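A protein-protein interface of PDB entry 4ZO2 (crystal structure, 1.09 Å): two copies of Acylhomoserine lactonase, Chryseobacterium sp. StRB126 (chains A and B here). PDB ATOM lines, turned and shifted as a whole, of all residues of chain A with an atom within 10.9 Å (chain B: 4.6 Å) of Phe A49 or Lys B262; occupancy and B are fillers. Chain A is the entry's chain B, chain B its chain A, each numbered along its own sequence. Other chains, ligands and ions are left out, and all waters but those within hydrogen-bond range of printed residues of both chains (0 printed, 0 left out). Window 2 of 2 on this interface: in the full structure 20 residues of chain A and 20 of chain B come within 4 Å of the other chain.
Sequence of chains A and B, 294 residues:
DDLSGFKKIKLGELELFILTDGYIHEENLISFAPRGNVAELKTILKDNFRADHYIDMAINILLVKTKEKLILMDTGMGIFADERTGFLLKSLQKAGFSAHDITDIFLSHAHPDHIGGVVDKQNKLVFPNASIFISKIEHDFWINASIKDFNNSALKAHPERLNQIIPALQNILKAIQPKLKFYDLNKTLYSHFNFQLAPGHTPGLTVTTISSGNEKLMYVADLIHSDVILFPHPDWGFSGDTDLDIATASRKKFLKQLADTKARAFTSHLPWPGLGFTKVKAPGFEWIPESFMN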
ATOM      1  N   LEU A  41      21.170  -5.630  10.946  1.00  0.00           N
ATOM      2  CA  LEU A  41      22.225  -6.107  10.072  1.00  0.00           C
ATOM      3  C   LEU A  41      21.698  -6.282   8.636  1.00  0.00           C
ATOM      4  O   LEU A  41      22.315  -5.829   7.672  1.00  0.00           O
ATOM      5  CB  LEU A  41      22.779  -7.422  10.625  1.00  0.00           C
ATOM      6  CG  LEU A  41      24.023  -7.948   9.914  1.00  0.00           C
ATOM      7  CD1 LEU A  41      25.010  -8.629  10.848  1.00  0.00           C
ATOM      8  CD2 LEU A  41      23.641  -8.878   8.800  1.00  0.00           C
ATOM      9  N   LYS A  42      20.571  -6.985   8.482  1.00  0.00           N
ATOM     10  CA  LYS A  42      20.044  -7.220   7.142  1.00  0.00           C
ATOM     11  C   LYS A  42      19.501  -5.930   6.514  1.00  0.00           C
ATOM     12  O   LYS A  42      19.632  -5.750   5.300  1.00  0.00           O
ATOM     13  CB  LYS A  42      19.001  -8.357   7.164  1.00  0.00           C
ATOM     14  CG  LYS A  42      19.671  -9.710   7.462  1.00  0.00           C
ATOM     15  CD  LYS A  42      18.813 -10.914   7.113  1.00  0.00           C
ATOM     16  CE  LYS A  42      19.537 -12.230   7.465  1.00  0.00           C
ATOM     17  NZ  LYS A  42      18.729 -13.434   7.095  1.00  0.00           N
ATOM     18  N   THR A  43      18.926  -5.027   7.308  1.00  0.00           N
ATOM     19  CA  THR A  43      18.521  -3.732   6.767  1.00  0.00           C
ATOM     20  C   THR A  43      19.710  -2.986   6.187  1.00  0.00           C
ATOM     21  O   THR A  43      19.612  -2.415   5.096  1.00  0.00           O
ATOM     22  CB  THR A  43      17.824  -2.891   7.846  1.00  0.00           C
ATOM     23  OG1 THR A  43      16.615  -3.567   8.220  1.00  0.00           O
ATOM     24  CG2 THR A  43      17.497  -1.488   7.332  1.00  0.00           C
ATOM     25  N   ILE A  44      20.825  -2.956   6.912  1.00  0.00           N
ATOM     26  CA  ILE A  44      21.998  -2.260   6.428  1.00  0.00           C
ATOM     27  C   ILE A  44      22.477  -2.868   5.102  1.00  0.00           C
ATOM     28  O   ILE A  44      22.825  -2.155   4.167  1.00  0.00           O
ATOM     29  CB  ILE A  44      23.129  -2.281   7.490  1.00  0.00           C
ATOM     30  CG1 ILE A  44      22.742  -1.448   8.715  1.00  0.00           C
ATOM     31  CG2 ILE A  44      24.431  -1.808   6.860  1.00  0.00           C
ATOM     32  CD1 ILE A  44      23.653  -1.662   9.897  1.00  0.00           C
ATOM     33  N   LEU A  45      22.515  -4.189   5.017  1.00  0.00           N
ATOM     34  CA  LEU A  45      22.940  -4.831   3.769  1.00  0.00           C
ATOM     35  C   LEU A  45      22.041  -4.400   2.616  1.00  0.00           C
ATOM     36  O   LEU A  45      22.542  -4.006   1.555  1.00  0.00           O
ATOM     37  CB  LEU A  45      22.966  -6.373   3.911  1.00  0.00           C
ATOM     38  CG  LEU A  45      24.039  -6.903   4.882  1.00  0.00           C
ATOM     39  CD1 LEU A  45      23.886  -8.413   5.035  1.00  0.00           C
ATOM     40  CD2 LEU A  45      25.441  -6.574   4.381  1.00  0.00           C
ATOM     41  N   LYS A  46      20.741  -4.455   2.822  1.00  0.00           N
ATOM     42  CA  LYS A  46      19.818  -4.066   1.765  1.00  0.00           C
ATOM     43  C   LYS A  46      19.868  -2.574   1.445  1.00  0.00           C
ATOM     44  O   LYS A  46      19.730  -2.191   0.276  1.00  0.00           O
ATOM     45  CB  LYS A  46      18.400  -4.484   2.126  1.00  0.00           C
ATOM     46  CG  LYS A  46      18.203  -5.996   1.988  1.00  0.00           C
ATOM     47  CD  LYS A  46      16.767  -6.460   2.158  1.00  0.00           C
ATOM     48  CE  LYS A  46      16.262  -6.155   3.544  1.00  0.00           C
ATOM     49  NZ  LYS A  46      16.912  -6.969   4.580  1.00  0.00           N
ATOM     50  N   ASP A  47      20.101  -1.731   2.451  1.00  0.00           N
ATOM     51  CA  ASP A  47      20.247  -0.293   2.210  1.00  0.00           C
ATOM     52  C   ASP A  47      21.457   0.018   1.353  1.00  0.00           C
ATOM     53  O   ASP A  47      21.548   1.098   0.784  1.00  0.00           O
ATOM     54  CB  ASP A  47      20.383   0.459   3.520  1.00  0.00           C
ATOM     55  CG  ASP A  47      19.075   0.577   4.281  1.00  0.00           C
ATOM     56  OD1 ASP A  47      18.006   0.290   3.717  1.00  0.00           O
ATOM     57  OD2 ASP A  47      19.130   0.978   5.459  1.00  0.00           O
ATOM     58  N   ASN A  48      22.399  -0.925   1.290  1.00  0.00           N
ATOM     59  CA  ASN A  48      23.566  -0.816   0.431  1.00  0.00           C
ATOM     60  C   ASN A  48      23.481  -1.692  -0.816  1.00  0.00           C
ATOM     61  O   ASN A  48      24.482  -1.856  -1.521  1.00  0.00           O
ATOM     62  CB  ASN A  48      24.828  -1.128   1.238  1.00  0.00           C
ATOM     63  CG  ASN A  48      25.185  -0.018   2.184  1.00  0.00           C
ATOM     64  OD1 ASN A  48      25.837   0.945   1.773  1.00  0.00           O
ATOM     65  ND2 ASN A  48      24.705  -0.084   3.420  1.00  0.00           N
ATOM     66  N   PHE A  49      22.279  -2.162  -1.131  1.00  0.00           N
ATOM     67  CA  PHE A  49      22.000  -2.900  -2.369  1.00  0.00           C
ATOM     68  C   PHE A  49      22.776  -4.205  -2.459  1.00  0.00           C
ATOM     69  O   PHE A  49      23.048  -4.691  -3.560  1.00  0.00           O
ATOM     70  CB  PHE A  49      22.243  -2.000  -3.614  1.00  0.00           C
ATOM     71  CG  PHE A  49      21.447  -0.745  -3.564  1.00  0.00           C
ATOM     72  CD1 PHE A  49      21.954   0.392  -2.931  1.00  0.00           C
ATOM     73  CD2 PHE A  49      20.189  -0.679  -4.137  1.00  0.00           C
ATOM     74  CE1 PHE A  49      21.210   1.564  -2.881  1.00  0.00           C
ATOM     75  CE2 PHE A  49      19.443   0.516  -4.074  1.00  0.00           C
ATOM     76  CZ  PHE A  49      19.965   1.620  -3.451  1.00  0.00           C
ATOM     77  N   ARG A  50      23.071  -4.787  -1.300  1.00  0.00           N
ATOM     78  CA  ARG A  50      23.734  -6.064  -1.214  1.00  0.00           C
ATOM     79  C   ARG A  50      22.749  -7.158  -0.835  1.00  0.00           C
ATOM     80  O   ARG A  50      21.695  -6.894  -0.278  1.00  0.00           O
ATOM     81  CB  ARG A  50      24.859  -6.006  -0.181  1.00  0.00           C
ATOM     82  CG  ARG A  50      25.840  -4.917  -0.489  1.00  0.00           C
ATOM     83  CD  ARG A  50      27.066  -4.961   0.360  1.00  0.00           C
ATOM     84  NE  ARG A  50      27.917  -3.791   0.130  1.00  0.00           N
ATOM     85  CZ  ARG A  50      28.989  -3.504   0.861  1.00  0.00           C
ATOM     86  NH1 ARG A  50      29.334  -4.297   1.860  1.00  0.00           N
ATOM     87  NH2 ARG A  50      29.684  -2.399   0.605  1.00  0.00           N
ATOM     88  N   ALA A  51      23.128  -8.399  -1.104  1.00  0.00           N
ATOM     89  CA  ALA A  51      22.399  -9.562  -0.618  1.00  0.00           C
ATOM     90  C   ALA A  51      22.251  -9.497   0.904  1.00  0.00           C
ATOM     91  O   ALA A  51      23.163  -9.014   1.605  1.00  0.00           O
ATOM     92  CB  ALA A  51      23.135 -10.814  -1.003  1.00  0.00           C
ATOM     93  N   ASP A  52      21.135  -9.997   1.426  1.00  0.00           N
ATOM     94  CA  ASP A  52      20.989 -10.007   2.883  1.00  0.00           C
ATOM     95  C   ASP A  52      21.075 -11.397   3.470  1.00  0.00           C
ATOM     96  O   ASP A  52      20.882 -11.546   4.666  1.00  0.00           O
ATOM     97  CB  ASP A  52      19.697  -9.320   3.320  1.00  0.00           C
ATOM     98  CG  ASP A  52      18.450 -10.140   3.028  1.00  0.00           C
ATOM     99  OD1 ASP A  52      18.508 -11.157   2.316  1.00  0.00           O
ATOM    100  OD2 ASP A  52      17.388  -9.752   3.546  1.00  0.00           O
ATOM    101  N   HIS A  53      21.434 -12.391   2.653  1.00  0.00           N
ATOM    102  CA  HIS A  53      21.478 -13.762   3.160  1.00  0.00           C
ATOM    103  C   HIS A  53      22.895 -14.341   3.149  1.00  0.00           C
ATOM    104  O   HIS A  53      23.088 -15.487   3.521  1.00  0.00           O
ATOM    105  CB  HIS A  53      20.486 -14.657   2.389  1.00  0.00           C
ATOM    106  CG  HIS A  53      20.784 -14.805   0.934  1.00  0.00           C
ATOM    107  ND1 HIS A  53      20.589 -13.787   0.023  1.00  0.00           N
ATOM    108  CD2 HIS A  53      21.251 -15.862   0.228  1.00  0.00           C
ATOM    109  CE1 HIS A  53      20.917 -14.217  -1.182  1.00  0.00           C
ATOM    110  NE2 HIS A  53      21.316 -15.472  -1.084  1.00  0.00           N
ATOM    111  N   TYR A  54      23.874 -13.532   2.769  1.00  0.00           N
ATOM    112  CA  TYR A  54      25.268 -13.891   2.907  1.00  0.00           C
ATOM    113  C   TYR A  54      26.061 -12.591   2.943  1.00  0.00           C
ATOM    114  O   TYR A  54      25.538 -11.542   2.557  1.00  0.00           O
ATOM    115  CB  TYR A  54      25.748 -14.803   1.752  1.00  0.00           C
ATOM    116  CG  TYR A  54      25.670 -14.159   0.386  1.00  0.00           C
ATOM    117  CD1 TYR A  54      26.690 -13.322  -0.076  1.00  0.00           C
ATOM    118  CD2 TYR A  54      24.591 -14.402  -0.462  1.00  0.00           C
ATOM    119  CE1 TYR A  54      26.618 -12.718  -1.335  1.00  0.00           C
ATOM    120  CE2 TYR A  54      24.518 -13.818  -1.724  1.00  0.00           C
ATOM    121  CZ  TYR A  54      25.528 -12.971  -2.156  1.00  0.00           C
ATOM    122  OH  TYR A  54      25.423 -12.381  -3.422  1.00  0.00           O
ATOM    123  N   ILE A  55      27.315 -12.686   3.368  1.00  0.00           N
ATOM    124  CA  ILE A  55      28.290 -11.601   3.250  1.00  0.00           C
ATOM    125  C   ILE A  55      29.534 -12.188   2.588  1.00  0.00           C
ATOM    126  O   ILE A  55      30.098 -13.161   3.071  1.00  0.00           O
ATOM    127  CB  ILE A  55      28.635 -10.976   4.618  1.00  0.00           C
ATOM    128  CG1 ILE A  55      27.423 -10.220   5.178  1.00  0.00           C
ATOM    129  CG2 ILE A  55      29.855 -10.078   4.502  1.00  0.00           C
ATOM    130  CD1 ILE A  55      27.614  -9.643   6.559  1.00  0.00           C
ATOM    131  N   ASP A  56      29.940 -11.597   1.475  1.00  0.00           N
ATOM    132  CA  ASP A  56      31.203 -11.950   0.843  1.00  0.00           C
ATOM    133  C   ASP A  56      32.321 -11.129   1.455  1.00  0.00           C
ATOM    134  O   ASP A  56      32.250  -9.892   1.452  1.00  0.00           O
ATOM    135  CB  ASP A  56      31.138 -11.717  -0.669  1.00  0.00           C
ATOM    136  CG  ASP A  56      30.356 -12.801  -1.391  1.00  0.00           C
ATOM    137  OD1 ASP A  56      30.203 -13.917  -0.846  1.00  0.00           O
ATOM    138  OD2 ASP A  56      29.916 -12.522  -2.520  1.00  0.00           O
ATOM    139  N   ASP A 227      32.579  -3.290   6.118  1.00  0.00           N
ATOM    140  CA  ASP A 227      32.539  -1.847   5.928  1.00  0.00           C
ATOM    141  C   ASP A 227      31.219  -1.265   6.421  1.00  0.00           C
ATOM    142  O   ASP A 227      31.214  -0.275   7.163  1.00  0.00           O
ATOM    143  CB  ASP A 227      32.830  -1.467   4.463  1.00  0.00           C
ATOM    144  CG  ASP A 227      31.950  -2.158   3.416  1.00  0.00           C
ATOM    145  OD1 ASP A 227      31.275  -3.172   3.679  1.00  0.00           O
ATOM    146  OD2 ASP A 227      31.936  -1.636   2.276  1.00  0.00           O
ATOM    147  N   VAL A 228      30.106  -1.859   6.028  1.00  0.00           N
ATOM    148  CA  VAL A 228      28.821  -1.234   6.314  1.00  0.00           C
ATOM    149  C   VAL A 228      28.227  -1.615   7.676  1.00  0.00           C
ATOM    150  O   VAL A 228      27.389  -0.860   8.202  1.00  0.00           O
ATOM    151  CB  VAL A 228      27.814  -1.519   5.169  1.00  0.00           C
ATOM    152  CG1 VAL A 228      28.298  -0.852   3.868  1.00  0.00           C
ATOM    153  CG2 VAL A 228      27.587  -3.004   4.961  1.00  0.00           C
ATOM    154  N   LEU B 258      16.139   5.543 -11.130  1.00  0.00           N
ATOM    155  CA  LEU B 258      17.099   4.578 -10.594  1.00  0.00           C
ATOM    156  C   LEU B 258      16.837   4.321  -9.120  1.00  0.00           C
ATOM    157  O   LEU B 258      16.904   3.180  -8.654  1.00  0.00           O
ATOM    158  CB  LEU B 258      18.531   5.065 -10.824  1.00  0.00           C
ATOM    159  CG  LEU B 258      18.964   5.057 -12.302  1.00  0.00           C
ATOM    160  CD1 LEU B 258      20.270   5.816 -12.433  1.00  0.00           C
ATOM    161  CD2 LEU B 258      19.107   3.653 -12.872  1.00  0.00           C
ATOM    162  N   ALA B 259      16.545   5.376  -8.364  1.00  0.00           N
ATOM    163  CA  ALA B 259      16.282   5.231  -6.934  1.00  0.00           C
ATOM    164  C   ALA B 259      15.008   4.427  -6.701  1.00  0.00           C
ATOM    165  O   ALA B 259      14.976   3.510  -5.873  1.00  0.00           O
ATOM    166  CB  ALA B 259      16.195   6.585  -6.263  1.00  0.00           C
ATOM    167  N   ASP B 260      13.952   4.784  -7.417  1.00  0.00           N
ATOM    168  CA  ASP B 260      12.656   4.155  -7.194  1.00  0.00           C
ATOM    169  C   ASP B 260      12.673   2.680  -7.571  1.00  0.00           C
ATOM    170  O   ASP B 260      11.996   1.861  -6.963  1.00  0.00           O
ATOM    171  CB  ASP B 260      11.580   4.858  -8.020  1.00  0.00           C
ATOM    172  CG  ASP B 260      11.228   6.239  -7.498  1.00  0.00           C
ATOM    173  OD1 ASP B 260      11.662   6.612  -6.377  1.00  0.00           O
ATOM    174  OD2 ASP B 260      10.511   6.951  -8.229  1.00  0.00           O
ATOM    175  N   THR B 261      13.447   2.341  -8.590  1.00  0.00           N
ATOM    176  CA  THR B 261      13.478   0.967  -9.075  1.00  0.00           C
ATOM    177  C   THR B 261      14.626   0.130  -8.495  1.00  0.00           C
ATOM    178  O   THR B 261      14.682  -1.083  -8.719  1.00  0.00           O
ATOM    179  CB  THR B 261      13.579   0.921 -10.618  1.00  0.00           C
ATOM    180  OG1 THR B 261      14.815   1.520 -11.044  1.00  0.00           O
ATOM    181  CG2 THR B 261      12.402   1.659 -11.266  1.00  0.00           C
ATOM    182  N   LYS B 262      15.522   0.766  -7.755  1.00  0.00           N
ATOM    183  CA  LYS B 262      16.715   0.126  -7.175  1.00  0.00           C
ATOM    184  C   LYS B 262      17.597  -0.508  -8.263  1.00  0.00           C
ATOM    185  O   LYS B 262      18.344  -1.449  -8.008  1.00  0.00           O
ATOM    186  CB  LYS B 262      16.338  -0.910  -6.100  1.00  0.00           C
ATOM    187  CG  LYS B 262      15.463  -0.321  -4.991  1.00  0.00           C
ATOM    188  CD  LYS B 262      15.209  -1.363  -3.907  1.00  0.00           C
ATOM    189  CE  LYS B 262      14.046  -1.008  -3.001  1.00  0.00           C
ATOM    190  NZ  LYS B 262      14.294   0.269  -2.305  1.00  0.00           N
ATOM    191  N   ALA B 263      17.549   0.058  -9.466  1.00  0.00           N
ATOM    192  CA  ALA B 263      18.267  -0.487 -10.605  1.00  0.00           C
ATOM    193  C   ALA B 263      19.748  -0.102 -10.622  1.00  0.00           C
ATOM    194  O   ALA B 263      20.137   1.003 -10.230  1.00  0.00           O
ATOM    195  CB  ALA B 263      17.590  -0.028 -11.904  1.00  0.00           C
ATOM    196  N   ARG B 264      20.565  -1.019 -11.139  1.00  0.00           N
ATOM    197  CA  ARG B 264      21.989  -0.766 -11.282  1.00  0.00           C
ATOM    198  C   ARG B 264      22.244   0.082 -12.539  1.00  0.00           C
ATOM    199  O   ARG B 264      21.638  -0.152 -13.592  1.00  0.00           O
ATOM    200  CB  ARG B 264      22.769  -2.082 -11.368  1.00  0.00           C
ATOM    201  CG  ARG B 264      24.276  -1.860 -11.342  1.00  0.00           C
ATOM    202  CD  ARG B 264      25.056  -3.158 -11.135  1.00  0.00           C
ATOM    203  NE  ARG B 264      24.729  -4.126 -12.178  1.00  0.00           N
ATOM    204  CZ  ARG B 264      25.525  -5.125 -12.562  1.00  0.00           C
ATOM    205  NH1 ARG B 264      26.750  -5.254 -12.051  1.00  0.00           N
ATOM    206  NH2 ARG B 264      25.119  -5.971 -13.497  1.00  0.00           N
ATOM    207  N   PHE B 277      24.472   1.996  -7.594  1.00  0.00           N
ATOM    208  CA  PHE B 277      23.062   2.127  -7.250  1.00  0.00           C
ATOM    209  C   PHE B 277      22.799   3.537  -6.755  1.00  0.00           C
ATOM    210  O   PHE B 277      23.716   4.212  -6.276  1.00  0.00           O
ATOM    211  CB  PHE B 277      22.699   1.090  -6.178  1.00  0.00           C
ATOM    212  CG  PHE B 277      22.929  -0.302  -6.635  1.00  0.00           C
ATOM    213  CD1 PHE B 277      21.927  -0.999  -7.284  1.00  0.00           C
ATOM    214  CD2 PHE B 277      24.154  -0.916  -6.438  1.00  0.00           C
ATOM    215  CE1 PHE B 277      22.135  -2.310  -7.726  1.00  0.00           C
ATOM    216  CE2 PHE B 277      24.371  -2.219  -6.866  1.00  0.00           C
ATOM    217  CZ  PHE B 277      23.351  -2.916  -7.510  1.00  0.00           C
ATOM    218  N   THR B 278      21.547   3.950  -6.849  1.00  0.00           N
ATOM    219  CA  THR B 278      21.159   5.303  -6.497  1.00  0.00           C
ATOM    220  C   THR B 278      20.122   5.252  -5.395  1.00  0.00           C
ATOM    221  O   THR B 278      19.149   4.490  -5.509  1.00  0.00           O
ATOM    222  CB  THR B 278      20.582   6.030  -7.734  1.00  0.00           C
ATOM    223  OG1 THR B 278      21.534   5.993  -8.793  1.00  0.00           O
ATOM    224  CG2 THR B 278      20.242   7.479  -7.440  1.00  0.00           C
ATOM    225  N   LYS B 279      20.303   6.070  -4.372  1.00  0.00           N
ATOM    226  CA  LYS B 279      19.357   6.149  -3.271  1.00  0.00           C
ATOM    227  C   LYS B 279      18.949   7.590  -3.045  1.00  0.00           C
ATOM    228  O   LYS B 279      19.770   8.492  -3.196  1.00  0.00           O
ATOM    229  CB  LYS B 279      19.979   5.566  -1.986  1.00  0.00           C
ATOM    230  CG  LYS B 279      18.977   5.241  -0.879  1.00  0.00           C
ATOM    231  CD  LYS B 279      19.527   4.157   0.016  1.00  0.00           C
ATOM    232  CE  LYS B 279      20.911   4.532   0.450  1.00  0.00           C
ATOM    233  NZ  LYS B 279      21.197   3.896   1.753  1.00  0.00           N
ATOM    234  N   ILE B 288      25.783   4.646  -4.454  1.00  0.00           N
ATOM    235  CA  ILE B 288      26.339   3.525  -3.707  1.00  0.00           C
ATOM    236  C   ILE B 288      27.093   2.666  -4.728  1.00  0.00           C
ATOM    237  O   ILE B 288      26.481   1.984  -5.546  1.00  0.00           O
ATOM    238  CB  ILE B 288      25.266   2.674  -3.004  1.00  0.00           C
ATOM    239  CG1 ILE B 288      24.330   3.536  -2.155  1.00  0.00           C
ATOM    240  CG2 ILE B 288      25.971   1.586  -2.156  1.00  0.00           C
ATOM    241  CD1 ILE B 288      25.015   4.249  -1.068  1.00  0.00           C
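The side-chain amino group of Lys B279 is in hydrogen-bond range of the backbone carbonyl oxygen of Asp A47, 3.0 Å away.
The backbone carbonyl oxygen (O) of Phe B277 sits at hydrogen-bond distance from the backbone NH (N) of Ile B288, at 2.8 Å.
O of Ile A44 is in hydrogen-bond range of ND2 of Asn A48 (2.9 Å).
Among the printed residues, merely in contact across the chains: Asn A48 with Ile B288 (3.8 Å), Phe A49 with Lys B262 (3.97 Å), Phe A49 with Phe B277 (3.4 Å), Phe A49 with Thr B278 (3.6 Å) and Phe A49 with Ile B288 (3.8 Å).
Printed residues of chain B within 4 Å of Asp A47: Lys B279.
Printed residues of chain B within 4 Å of Asn A48: Ile B288.
Of the printed residues of chain B, Phe A49 touches Lys B262 (3.97 Å), Phe B277 (3.4 Å), Thr B278 (3.6 Å) and Ile B288 (3.8 Å).
Arg A50 touches none of the printed residues of chain B.
No residue of chain A comes within 4 Å of Thr B261.
Of chain A, only Phe A49 (3.97 Å) comes within 4 Å of Lys B262.
No residue of chain A comes within 4 Å of Ala B263.
Phe B277 touches one residue of chain A.
Of the printed residues of chain A, Thr B278 touches Phe A49.
The nearest printed residue of chain B that does not touch Phe A49 is Lys B279 (4.2 Å).
Of the 11 printed residues of chain B, 5 touch a printed residue of chain A.
Along chain A the printed residues that touch a printed residue of chain B span positions 47 to 49.
No position is printed for both chains.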
